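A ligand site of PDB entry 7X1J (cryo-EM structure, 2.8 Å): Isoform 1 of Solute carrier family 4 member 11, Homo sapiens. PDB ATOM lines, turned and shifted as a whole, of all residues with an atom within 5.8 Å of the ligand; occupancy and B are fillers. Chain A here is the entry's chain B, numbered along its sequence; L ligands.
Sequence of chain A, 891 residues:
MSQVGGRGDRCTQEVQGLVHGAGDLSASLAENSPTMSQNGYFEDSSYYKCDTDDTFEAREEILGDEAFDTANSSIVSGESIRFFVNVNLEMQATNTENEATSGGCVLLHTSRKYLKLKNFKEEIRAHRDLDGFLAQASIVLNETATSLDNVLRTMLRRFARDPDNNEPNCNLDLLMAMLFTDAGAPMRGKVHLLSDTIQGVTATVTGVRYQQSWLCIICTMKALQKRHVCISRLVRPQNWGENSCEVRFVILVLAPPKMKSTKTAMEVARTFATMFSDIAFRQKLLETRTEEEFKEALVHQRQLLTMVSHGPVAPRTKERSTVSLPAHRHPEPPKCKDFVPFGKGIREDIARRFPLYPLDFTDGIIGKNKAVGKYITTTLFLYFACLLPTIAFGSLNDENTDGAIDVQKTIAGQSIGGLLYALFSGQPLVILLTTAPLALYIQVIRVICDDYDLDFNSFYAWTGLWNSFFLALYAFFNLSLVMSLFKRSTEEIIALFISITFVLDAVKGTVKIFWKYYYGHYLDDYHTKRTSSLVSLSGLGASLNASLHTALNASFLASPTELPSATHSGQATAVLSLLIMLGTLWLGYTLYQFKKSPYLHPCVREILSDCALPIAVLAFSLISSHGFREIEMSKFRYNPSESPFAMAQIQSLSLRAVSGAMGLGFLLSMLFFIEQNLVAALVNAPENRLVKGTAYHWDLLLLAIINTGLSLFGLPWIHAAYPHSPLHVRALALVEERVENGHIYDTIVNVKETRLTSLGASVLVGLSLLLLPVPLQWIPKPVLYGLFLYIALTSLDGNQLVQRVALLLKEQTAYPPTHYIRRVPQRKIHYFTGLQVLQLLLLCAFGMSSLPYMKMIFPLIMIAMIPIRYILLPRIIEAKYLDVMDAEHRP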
ATOM      1  N   ARG A 125      24.678 -34.802  18.210  1.00  0.00           N
ATOM      2  CA  ARG A 125      25.322 -34.503  19.479  1.00  0.00           C
ATOM      3  C   ARG A 125      25.874 -35.777  20.115  1.00  0.00           C
ATOM      4  O   ARG A 125      26.911 -35.746  20.745  1.00  0.00           O
ATOM      5  CB  ARG A 125      24.359 -33.778  20.421  1.00  0.00           C
ATOM      6  CG  ARG A 125      25.060 -33.059  21.554  1.00  0.00           C
ATOM      7  CD  ARG A 125      26.221 -32.248  21.027  1.00  0.00           C
ATOM      8  NE  ARG A 125      27.243 -32.102  22.052  1.00  0.00           N
ATOM      9  CZ  ARG A 125      28.450 -31.592  21.854  1.00  0.00           C
ATOM     10  NH1 ARG A 125      28.814 -31.191  20.660  1.00  0.00           N
ATOM     11  NH2 ARG A 125      29.291 -31.506  22.851  1.00  0.00           N
ATOM     12  N   ARG A 128      29.163 -36.269  18.563  1.00  0.00           N
ATOM     13  CA  ARG A 128      30.111 -35.268  19.026  1.00  0.00           C
ATOM     14  C   ARG A 128      30.567 -35.553  20.453  1.00  0.00           C
ATOM     15  O   ARG A 128      31.759 -35.442  20.762  1.00  0.00           O
ATOM     16  CB  ARG A 128      29.494 -33.870  18.924  1.00  0.00           C
ATOM     17  CG  ARG A 128      29.795 -33.180  17.606  1.00  0.00           C
ATOM     18  CD  ARG A 128      29.022 -31.876  17.465  1.00  0.00           C
ATOM     19  NE  ARG A 128      29.529 -31.066  16.358  1.00  0.00           N
ATOM     20  CZ  ARG A 128      29.212 -31.265  15.086  1.00  0.00           C
ATOM     21  NH1 ARG A 128      28.409 -32.249  14.719  1.00  0.00           N
ATOM     22  NH2 ARG A 128      29.724 -30.465  14.158  1.00  0.00           N
ATOM     23  N   ASP A 129      29.639 -35.937  21.335  1.00  0.00           N
ATOM     24  CA  ASP A 129      30.006 -36.268  22.711  1.00  0.00           C
ATOM     25  C   ASP A 129      30.901 -37.503  22.769  1.00  0.00           C
ATOM     26  O   ASP A 129      31.852 -37.539  23.549  1.00  0.00           O
ATOM     27  CB  ASP A 129      28.744 -36.472  23.557  1.00  0.00           C
ATOM     28  CG  ASP A 129      27.963 -35.194  23.764  1.00  0.00           C
ATOM     29  OD1 ASP A 129      28.586 -34.116  23.821  1.00  0.00           O
ATOM     30  OD2 ASP A 129      26.719 -35.269  23.861  1.00  0.00           O
ATOM     31  N   ARG A 227      33.084 -30.666  30.150  1.00  0.00           N
ATOM     32  CA  ARG A 227      32.306 -31.850  30.480  1.00  0.00           C
ATOM     33  C   ARG A 227      33.255 -33.036  30.609  1.00  0.00           C
ATOM     34  O   ARG A 227      33.993 -33.353  29.666  1.00  0.00           O
ATOM     35  CB  ARG A 227      31.241 -32.117  29.416  1.00  0.00           C
ATOM     36  CG  ARG A 227      30.301 -30.954  29.180  1.00  0.00           C
ATOM     37  CD  ARG A 227      29.371 -31.248  28.012  1.00  0.00           C
ATOM     38  NE  ARG A 227      30.104 -31.641  26.819  1.00  0.00           N
ATOM     39  CZ  ARG A 227      30.622 -30.787  25.937  1.00  0.00           C
ATOM     40  NH1 ARG A 227      30.496 -29.477  26.086  1.00  0.00           N
ATOM     41  NH2 ARG A 227      31.280 -31.259  24.892  1.00  0.00           N
ATOM     42  N   LYS A 260      24.625 -25.600  26.817  1.00  0.00           N
ATOM     43  CA  LYS A 260      23.520 -25.684  25.860  1.00  0.00           C
ATOM     44  C   LYS A 260      22.585 -26.827  26.209  1.00  0.00           C
ATOM     45  O   LYS A 260      22.992 -27.849  26.763  1.00  0.00           O
ATOM     46  CB  LYS A 260      24.062 -25.871  24.445  1.00  0.00           C
ATOM     47  CG  LYS A 260      25.167 -24.906  24.061  1.00  0.00           C
ATOM     48  CD  LYS A 260      25.670 -25.183  22.652  1.00  0.00           C
ATOM     49  CE  LYS A 260      24.540 -25.076  21.637  1.00  0.00           C
ATOM     50  NZ  LYS A 260      25.009 -25.359  20.251  1.00  0.00           N
ATOM     51  N   THR A 262      21.307 -29.005  24.452  1.00  0.00           N
ATOM     52  CA  THR A 262      21.619 -30.257  23.771  1.00  0.00           C
ATOM     53  C   THR A 262      22.845 -30.957  24.350  1.00  0.00           C
ATOM     54  O   THR A 262      23.066 -32.128  24.036  1.00  0.00           O
ATOM     55  CB  THR A 262      21.838 -30.008  22.271  1.00  0.00           C
ATOM     56  OG1 THR A 262      22.927 -29.096  22.101  1.00  0.00           O
ATOM     57  CG2 THR A 262      20.586 -29.431  21.644  1.00  0.00           C
ATOM     58  N   LYS A 263      23.648 -30.247  25.124  1.00  0.00           N
ATOM     59  CA  LYS A 263      24.833 -30.840  25.736  1.00  0.00           C
ATOM     60  C   LYS A 263      24.877 -30.674  27.248  1.00  0.00           C
ATOM     61  O   LYS A 263      25.943 -30.487  27.820  1.00  0.00           O
ATOM     62  CB  LYS A 263      26.128 -30.366  25.073  1.00  0.00           C
ATOM     63  CG  LYS A 263      26.354 -28.873  24.998  1.00  0.00           C
ATOM     64  CD  LYS A 263      27.422 -28.579  23.966  1.00  0.00           C
ATOM     65  CE  LYS A 263      28.160 -27.284  24.261  1.00  0.00           C
ATOM     66  NZ  LYS A 263      28.928 -26.809  23.084  1.00  0.00           N
ATOM     67  N   VAL A 805      17.882 -16.135  12.373  1.00  0.00           N
ATOM     68  CA  VAL A 805      18.625 -14.876  12.304  1.00  0.00           C
ATOM     69  C   VAL A 805      18.918 -14.369  13.711  1.00  0.00           C
ATOM     70  O   VAL A 805      20.053 -13.951  14.009  1.00  0.00           O
ATOM     71  CB  VAL A 805      17.855 -13.837  11.474  1.00  0.00           C
ATOM     72  CG1 VAL A 805      18.424 -12.444  11.692  1.00  0.00           C
ATOM     73  CG2 VAL A 805      17.902 -14.196   9.994  1.00  0.00           C
ATOM     74  N   LEU A 808      21.734 -16.383  15.338  1.00  0.00           N
ATOM     75  CA  LEU A 808      23.112 -16.069  14.964  1.00  0.00           C
ATOM     76  C   LEU A 808      23.634 -15.216  16.058  1.00  0.00           C
ATOM     77  O   LEU A 808      24.698 -15.474  16.618  1.00  0.00           O
ATOM     78  CB  LEU A 808      23.157 -15.287  13.660  1.00  0.00           C
ATOM     79  CG  LEU A 808      22.737 -15.962  12.363  1.00  0.00           C
ATOM     80  CD1 LEU A 808      22.520 -14.908  11.289  1.00  0.00           C
ATOM     81  CD2 LEU A 808      23.800 -16.948  11.929  1.00  0.00           C
ATOM     82  N   LEU A 809      22.893 -14.166  16.359  1.00  0.00           N
ATOM     83  CA  LEU A 809      23.266 -13.312  17.451  1.00  0.00           C
ATOM     84  C   LEU A 809      22.645 -13.895  18.687  1.00  0.00           C
ATOM     85  O   LEU A 809      21.639 -13.377  19.139  1.00  0.00           O
ATOM     86  CB  LEU A 809      22.712 -11.912  17.234  1.00  0.00           C
ATOM     87  CG  LEU A 809      22.924 -11.307  15.848  1.00  0.00           C
ATOM     88  CD1 LEU A 809      22.014 -10.116  15.643  1.00  0.00           C
ATOM     89  CD2 LEU A 809      24.388 -10.930  15.644  1.00  0.00           C
ATOM     90  N   LYS A 810      23.202 -14.977  19.234  1.00  0.00           N
ATOM     91  CA  LYS A 810      22.733 -15.521  20.512  1.00  0.00           C
ATOM     92  C   LYS A 810      23.909 -16.216  21.168  1.00  0.00           C
ATOM     93  O   LYS A 810      24.751 -16.781  20.482  1.00  0.00           O
ATOM     94  CB  LYS A 810      21.547 -16.473  20.340  1.00  0.00           C
ATOM     95  CG  LYS A 810      20.802 -16.793  21.615  1.00  0.00           C
ATOM     96  CD  LYS A 810      19.442 -17.387  21.311  1.00  0.00           C
ATOM     97  CE  LYS A 810      18.583 -16.394  20.556  1.00  0.00           C
ATOM     98  NZ  LYS A 810      17.254 -16.964  20.222  1.00  0.00           N
ATOM     99  N   GLN A 812      25.847 -19.154  22.999  1.00  0.00           N
ATOM    100  CA  GLN A 812      25.669 -20.588  22.814  1.00  0.00           C
ATOM    101  C   GLN A 812      24.790 -21.196  23.871  1.00  0.00           C
ATOM    102  O   GLN A 812      23.942 -22.028  23.566  1.00  0.00           O
ATOM    103  CB  GLN A 812      27.013 -21.290  22.767  1.00  0.00           C
ATOM    104  CG  GLN A 812      27.882 -20.874  21.598  1.00  0.00           C
ATOM    105  CD  GLN A 812      27.285 -21.271  20.263  1.00  0.00           C
ATOM    106  OE1 GLN A 812      26.757 -22.376  20.113  1.00  0.00           O
ATOM    107  NE2 GLN A 812      27.377 -20.386  19.284  1.00  0.00           N
ATOM    108  N   TYR A 815      20.932 -21.342  23.294  1.00  0.00           N
ATOM    109  CA  TYR A 815      20.355 -22.024  22.132  1.00  0.00           C
ATOM    110  C   TYR A 815      19.239 -22.965  22.574  1.00  0.00           C
ATOM    111  O   TYR A 815      19.469 -23.845  23.411  1.00  0.00           O
ATOM    112  CB  TYR A 815      21.443 -22.810  21.390  1.00  0.00           C
ATOM    113  CG  TYR A 815      22.208 -21.998  20.383  1.00  0.00           C
ATOM    114  CD1 TYR A 815      22.772 -20.771  20.727  1.00  0.00           C
ATOM    115  CD2 TYR A 815      22.392 -22.456  19.090  1.00  0.00           C
ATOM    116  CE1 TYR A 815      23.484 -20.030  19.802  1.00  0.00           C
ATOM    117  CE2 TYR A 815      23.099 -21.719  18.156  1.00  0.00           C
ATOM    118  CZ  TYR A 815      23.644 -20.504  18.531  1.00  0.00           C
ATOM    119  OH  TYR A 815      24.355 -19.763  17.605  1.00  0.00           O
ATOM    120  N   GLN A 826      25.339 -26.828  13.607  1.00  0.00           N
ATOM    121  CA  GLN A 826      25.179 -25.389  13.735  1.00  0.00           C
ATOM    122  C   GLN A 826      25.809 -24.672  12.577  1.00  0.00           C
ATOM    123  O   GLN A 826      25.259 -23.708  12.062  1.00  0.00           O
ATOM    124  CB  GLN A 826      25.841 -24.944  15.033  1.00  0.00           C
ATOM    125  CG  GLN A 826      25.675 -23.477  15.378  1.00  0.00           C
ATOM    126  CD  GLN A 826      26.390 -23.118  16.663  1.00  0.00           C
ATOM    127  OE1 GLN A 826      26.332 -21.985  17.117  1.00  0.00           O
ATOM    128  NE2 GLN A 826      27.070 -24.099  17.251  1.00  0.00           N
ATOM    129  N   ARG A 827      26.976 -25.133  12.180  1.00  0.00           N
ATOM    130  CA  ARG A 827      27.664 -24.520  11.042  1.00  0.00           C
ATOM    131  C   ARG A 827      26.807 -24.591   9.780  1.00  0.00           C
ATOM    132  O   ARG A 827      26.730 -23.623   9.023  1.00  0.00           O
ATOM    133  CB  ARG A 827      29.016 -25.210  10.818  1.00  0.00           C
ATOM    134  CG  ARG A 827      29.752 -24.731   9.582  1.00  0.00           C
ATOM    135  CD  ARG A 827      31.127 -25.378   9.475  1.00  0.00           C
ATOM    136  NE  ARG A 827      32.002 -24.963  10.561  1.00  0.00           N
ATOM    137  CZ  ARG A 827      32.796 -23.906  10.516  1.00  0.00           C
ATOM    138  NH1 ARG A 827      32.862 -23.131   9.444  1.00  0.00           N
ATOM    139  NH2 ARG A 827      33.560 -23.619  11.568  1.00  0.00           N
ATOM    140  N   HIS A 830      23.740 -22.122  10.147  1.00  0.00           N
ATOM    141  CA  HIS A 830      24.086 -20.735   9.890  1.00  0.00           C
ATOM    142  C   HIS A 830      24.361 -20.492   8.411  1.00  0.00           C
ATOM    143  O   HIS A 830      24.029 -19.427   7.881  1.00  0.00           O
ATOM    144  CB  HIS A 830      25.289 -20.332  10.740  1.00  0.00           C
ATOM    145  CG  HIS A 830      25.003 -20.274  12.210  1.00  0.00           C
ATOM    146  ND1 HIS A 830      23.733 -20.459  12.721  1.00  0.00           N
ATOM    147  CD2 HIS A 830      25.817 -20.068  13.262  1.00  0.00           C
ATOM    148  CE1 HIS A 830      23.779 -20.355  14.036  1.00  0.00           C
ATOM    149  NE2 HIS A 830      25.033 -20.124  14.398  1.00  0.00           N
ATOM    150  N   TYR A 831      24.959 -21.465   7.723  1.00  0.00           N
ATOM    151  CA  TYR A 831      25.112 -21.367   6.276  1.00  0.00           C
ATOM    152  C   TYR A 831      23.756 -21.324   5.592  1.00  0.00           C
ATOM    153  O   TYR A 831      23.550 -20.523   4.666  1.00  0.00           O
ATOM    154  CB  TYR A 831      25.937 -22.546   5.751  1.00  0.00           C
ATOM    155  CG  TYR A 831      27.401 -22.505   6.113  1.00  0.00           C
ATOM    156  CD1 TYR A 831      27.981 -21.356   6.628  1.00  0.00           C
ATOM    157  CD2 TYR A 831      28.203 -23.623   5.938  1.00  0.00           C
ATOM    158  CE1 TYR A 831      29.316 -21.312   6.963  1.00  0.00           C
ATOM    159  CE2 TYR A 831      29.544 -23.593   6.264  1.00  0.00           C
ATOM    160  CZ  TYR A 831      30.101 -22.438   6.777  1.00  0.00           C
ATOM    161  OH  TYR A 831      31.433 -22.407   7.107  1.00  0.00           O
ATOM    162  N   THR A 833      20.958 -20.281   6.965  1.00  0.00           N
ATOM    163  CA  THR A 833      20.389 -18.969   7.284  1.00  0.00           C
ATOM    164  C   THR A 833      20.994 -17.886   6.397  1.00  0.00           C
ATOM    165  O   THR A 833      20.265 -17.022   5.886  1.00  0.00           O
ATOM    166  CB  THR A 833      20.620 -18.641   8.756  1.00  0.00           C
ATOM    167  OG1 THR A 833      20.034 -19.668   9.564  1.00  0.00           O
ATOM    168  CG2 THR A 833      19.982 -17.300   9.113  1.00  0.00           C
ATOM    169  N   GLY A 834      22.304 -17.916   6.189  1.00  0.00           N
ATOM    170  CA  GLY A 834      22.944 -16.921   5.339  1.00  0.00           C
ATOM    171  C   GLY A 834      22.476 -17.007   3.894  1.00  0.00           C
ATOM    172  O   GLY A 834      22.261 -15.976   3.250  1.00  0.00           O
ATOM    173  N   VAL A 837      19.041 -15.464   3.634  1.00  0.00           N
ATOM    174  CA  VAL A 837      19.140 -14.004   3.625  1.00  0.00           C
ATOM    175  C   VAL A 837      19.586 -13.516   2.250  1.00  0.00           C
ATOM    176  O   VAL A 837      19.097 -12.491   1.755  1.00  0.00           O
ATOM    177  CB  VAL A 837      20.091 -13.524   4.735  1.00  0.00           C
ATOM    178  CG1 VAL A 837      20.311 -12.026   4.647  1.00  0.00           C
ATOM    179  CG2 VAL A 837      19.538 -13.898   6.102  1.00  0.00           C
HETATM  180  O1  LIG L   1      33.771 -24.798  14.157  1.00  0.00           O
HETATM  181  P1  LIG L   1      32.406 -25.068  14.654  1.00  0.00           P
HETATM  182  O2  LIG L   1      31.863 -23.853  15.527  1.00  0.00           O
HETATM  183  O3  LIG L   1      31.366 -25.369  13.580  1.00  0.00           O
HETATM  184  O4  LIG L   1      29.705 -26.748  16.431  1.00  0.00           O
HETATM  185  O5  LIG L   1      32.368 -26.273  15.663  1.00  0.00           O
HETATM  186  C1  LIG L   1      32.016 -26.446  17.050  1.00  0.00           C
HETATM  187  C2  LIG L   1      30.787 -27.322  17.144  1.00  0.00           C
HETATM  188  C3  LIG L   1      33.198 -27.061  17.788  1.00  0.00           C
HETATM  189  O6  LIG L   1      34.359 -26.269  17.625  1.00  0.00           O
HETATM  190  C4  LIG L   1      32.851 -27.185  19.261  1.00  0.00           C
HETATM  191  O7  LIG L   1      33.935 -27.787  19.962  1.00  0.00           O
HETATM  192  C5  LIG L   1      31.577 -28.012  19.433  1.00  0.00           C
HETATM  193  O8  LIG L   1      31.215 -28.005  20.834  1.00  0.00           O
HETATM  194  P2  LIG L   1      31.790 -28.935  22.002  1.00  0.00           P
HETATM  195  O9  LIG L   1      33.187 -28.556  22.306  1.00  0.00           O
HETATM  196  O10 LIG L   1      31.652 -30.373  21.491  1.00  0.00           O
HETATM  197  O11 LIG L   1      30.847 -28.743  23.180  1.00  0.00           O
HETATM  198  C6  LIG L   1      30.432 -27.455  18.626  1.00  0.00           C
HETATM  199  O12 LIG L   1      29.296 -28.340  18.746  1.00  0.00           O
HETATM  200  P3  LIG L   1      27.865 -27.921  19.358  1.00  0.00           P
HETATM  201  O13 LIG L   1      28.021 -26.768  20.272  1.00  0.00           O
HETATM  202  O14 LIG L   1      26.957 -27.637  18.173  1.00  0.00           O
HETATM  203  O15 LIG L   1      27.340 -29.160  20.063  1.00  0.00           O
HETATM  204  C7  LIG L   1      31.498 -22.552  15.022  1.00  0.00           C
HETATM  205  C8  LIG L   1      30.068 -22.600  14.554  1.00  0.00           C
HETATM  206  C9  LIG L   1      29.163 -21.683  15.337  1.00  0.00           C
HETATM  207  O16 LIG L   1      30.013 -22.321  13.111  1.00  0.00           O
HETATM  208  C10 LIG L   1      30.198 -21.072  12.664  1.00  0.00           C
HETATM  209  O17 LIG L   1      31.216 -20.459  12.817  1.00  0.00           O
HETATM  210  O18 LIG L   1      29.658 -20.329  15.340  1.00  0.00           O
HETATM  211  C11 LIG L   1      28.997 -19.444  16.072  1.00  0.00           C
HETATM  212  O19 LIG L   1      28.211 -19.751  16.933  1.00  0.00           O
HETATM  213  C12 LIG L   1      28.988 -20.566  11.936  1.00  0.00           C
HETATM  214  C13 LIG L   1      29.256 -20.251  10.474  1.00  0.00           C
HETATM  215  C14 LIG L   1      29.964 -18.925  10.264  1.00  0.00           C
HETATM  216  C15 LIG L   1      29.300 -18.036   9.233  1.00  0.00           C
HETATM  217  C16 LIG L   1      27.913 -17.554   9.622  1.00  0.00           C
HETATM  218  C17 LIG L   1      27.215 -16.755   8.543  1.00  0.00           C
HETATM  219  C18 LIG L   1      25.917 -16.089   9.000  1.00  0.00           C
HETATM  220  C19 LIG L   1      25.168 -15.438   7.875  1.00  0.00           C
HETATM  221  C20 LIG L   1      25.119 -14.149   7.621  1.00  0.00           C
HETATM  222  C21 LIG L   1      24.498 -13.093   8.483  1.00  0.00           C
HETATM  223  C22 LIG L   1      23.131 -12.653   7.982  1.00  0.00           C
HETATM  224  C23 LIG L   1      22.526 -11.504   8.774  1.00  0.00           C
HETATM  225  C24 LIG L   1      21.172 -11.038   8.251  1.00  0.00           C
HETATM  226  C25 LIG L   1      29.308 -18.040  15.662  1.00  0.00           C
HETATM  227  C26 LIG L   1      28.182 -17.395  14.875  1.00  0.00           C
HETATM  228  C27 LIG L   1      28.582 -16.058  14.283  1.00  0.00           C
HETATM  229  C28 LIG L   1      27.470 -15.378  13.495  1.00  0.00           C
HETATM  230  C29 LIG L   1      27.884 -14.047  12.885  1.00  0.00           C
HETATM  231  C30 LIG L   1      26.716 -13.240  12.331  1.00  0.00           C
HETATM  232  C31 LIG L   1      27.116 -11.903  11.738  1.00  0.00           C
HETATM  233  C32 LIG L   1      25.942 -11.064  11.337  1.00  0.00           C
HETATM  234  C33 LIG L   1      20.621  -9.809   8.958  1.00  0.00           C
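NE2 of His 830 is in hydrogen-bond range of OH of Tyr 815, 3.3 Å away.
OE1 of Gln 812 lies within hydrogen-bond range of NZ of Lys 260, 3.5 Å away.
The side-chain amide nitrogen (NE2) of Gln 812 sits at hydrogen-bond distance from the side-chain amide oxygen (OE1) of Gln 826, 2.9 Å away.
The guanidinium group (NH1) of Arg 827 lies within hydrogen-bond range of the side-chain hydroxyl (OH) of Tyr 831, at 2.8 Å.
The side-chain hydroxyl (OH) of Tyr 815 lies within hydrogen-bond range of the side-chain amide oxygen (OE1) of Gln 826 (3.0 Å).
The guanidinium group (NH2) of Arg 125 lies within salt-bridge range of the side-chain carboxylate (OD1) of Asp 129 (2.9 Å).
Merely in contact with the ligand: Arg 128, Leu 808, Tyr 815, His 830, Tyr 831, Gly 834 and Val 837.
Hydrophobic or aromatic side chains within 4 Å of the ligand: Leu 808, His 830, Tyr 831 and Val 837.
Within 4 Å of the ligand: Arg 125, Arg 128, Arg 227, Lys 260, Lys 263, Leu 808, Gln 812, Tyr 815, Gln 826, Arg 827, His 830, Tyr 831, Gly 834 and Val 837.
The side-chain amide oxygen of Gln 826 sits close to an oxygen (O19) of the ligand, at 2.9 Å.
O11 of the ligand is in salt-bridge range of NH1 of Arg 227, at 3.0 Å.
O1 of the ligand is in salt-bridge range of NH2 of Arg 827.
The side-chain amide nitrogen of Gln 812 lies within hydrogen-bond range of an oxygen (O19) of the ligand.
NZ of Lys 260 is in salt-bridge range of O13 of the ligand.
The guanidinium group (NH1) of Arg 125 is in salt-bridge range of an oxygen (O15) of the ligand (2.6 Å).
The side-chain amino group (NZ) of Lys 263 lies within salt-bridge range of an oxygen (O11) of the ligand (2.7 Å).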
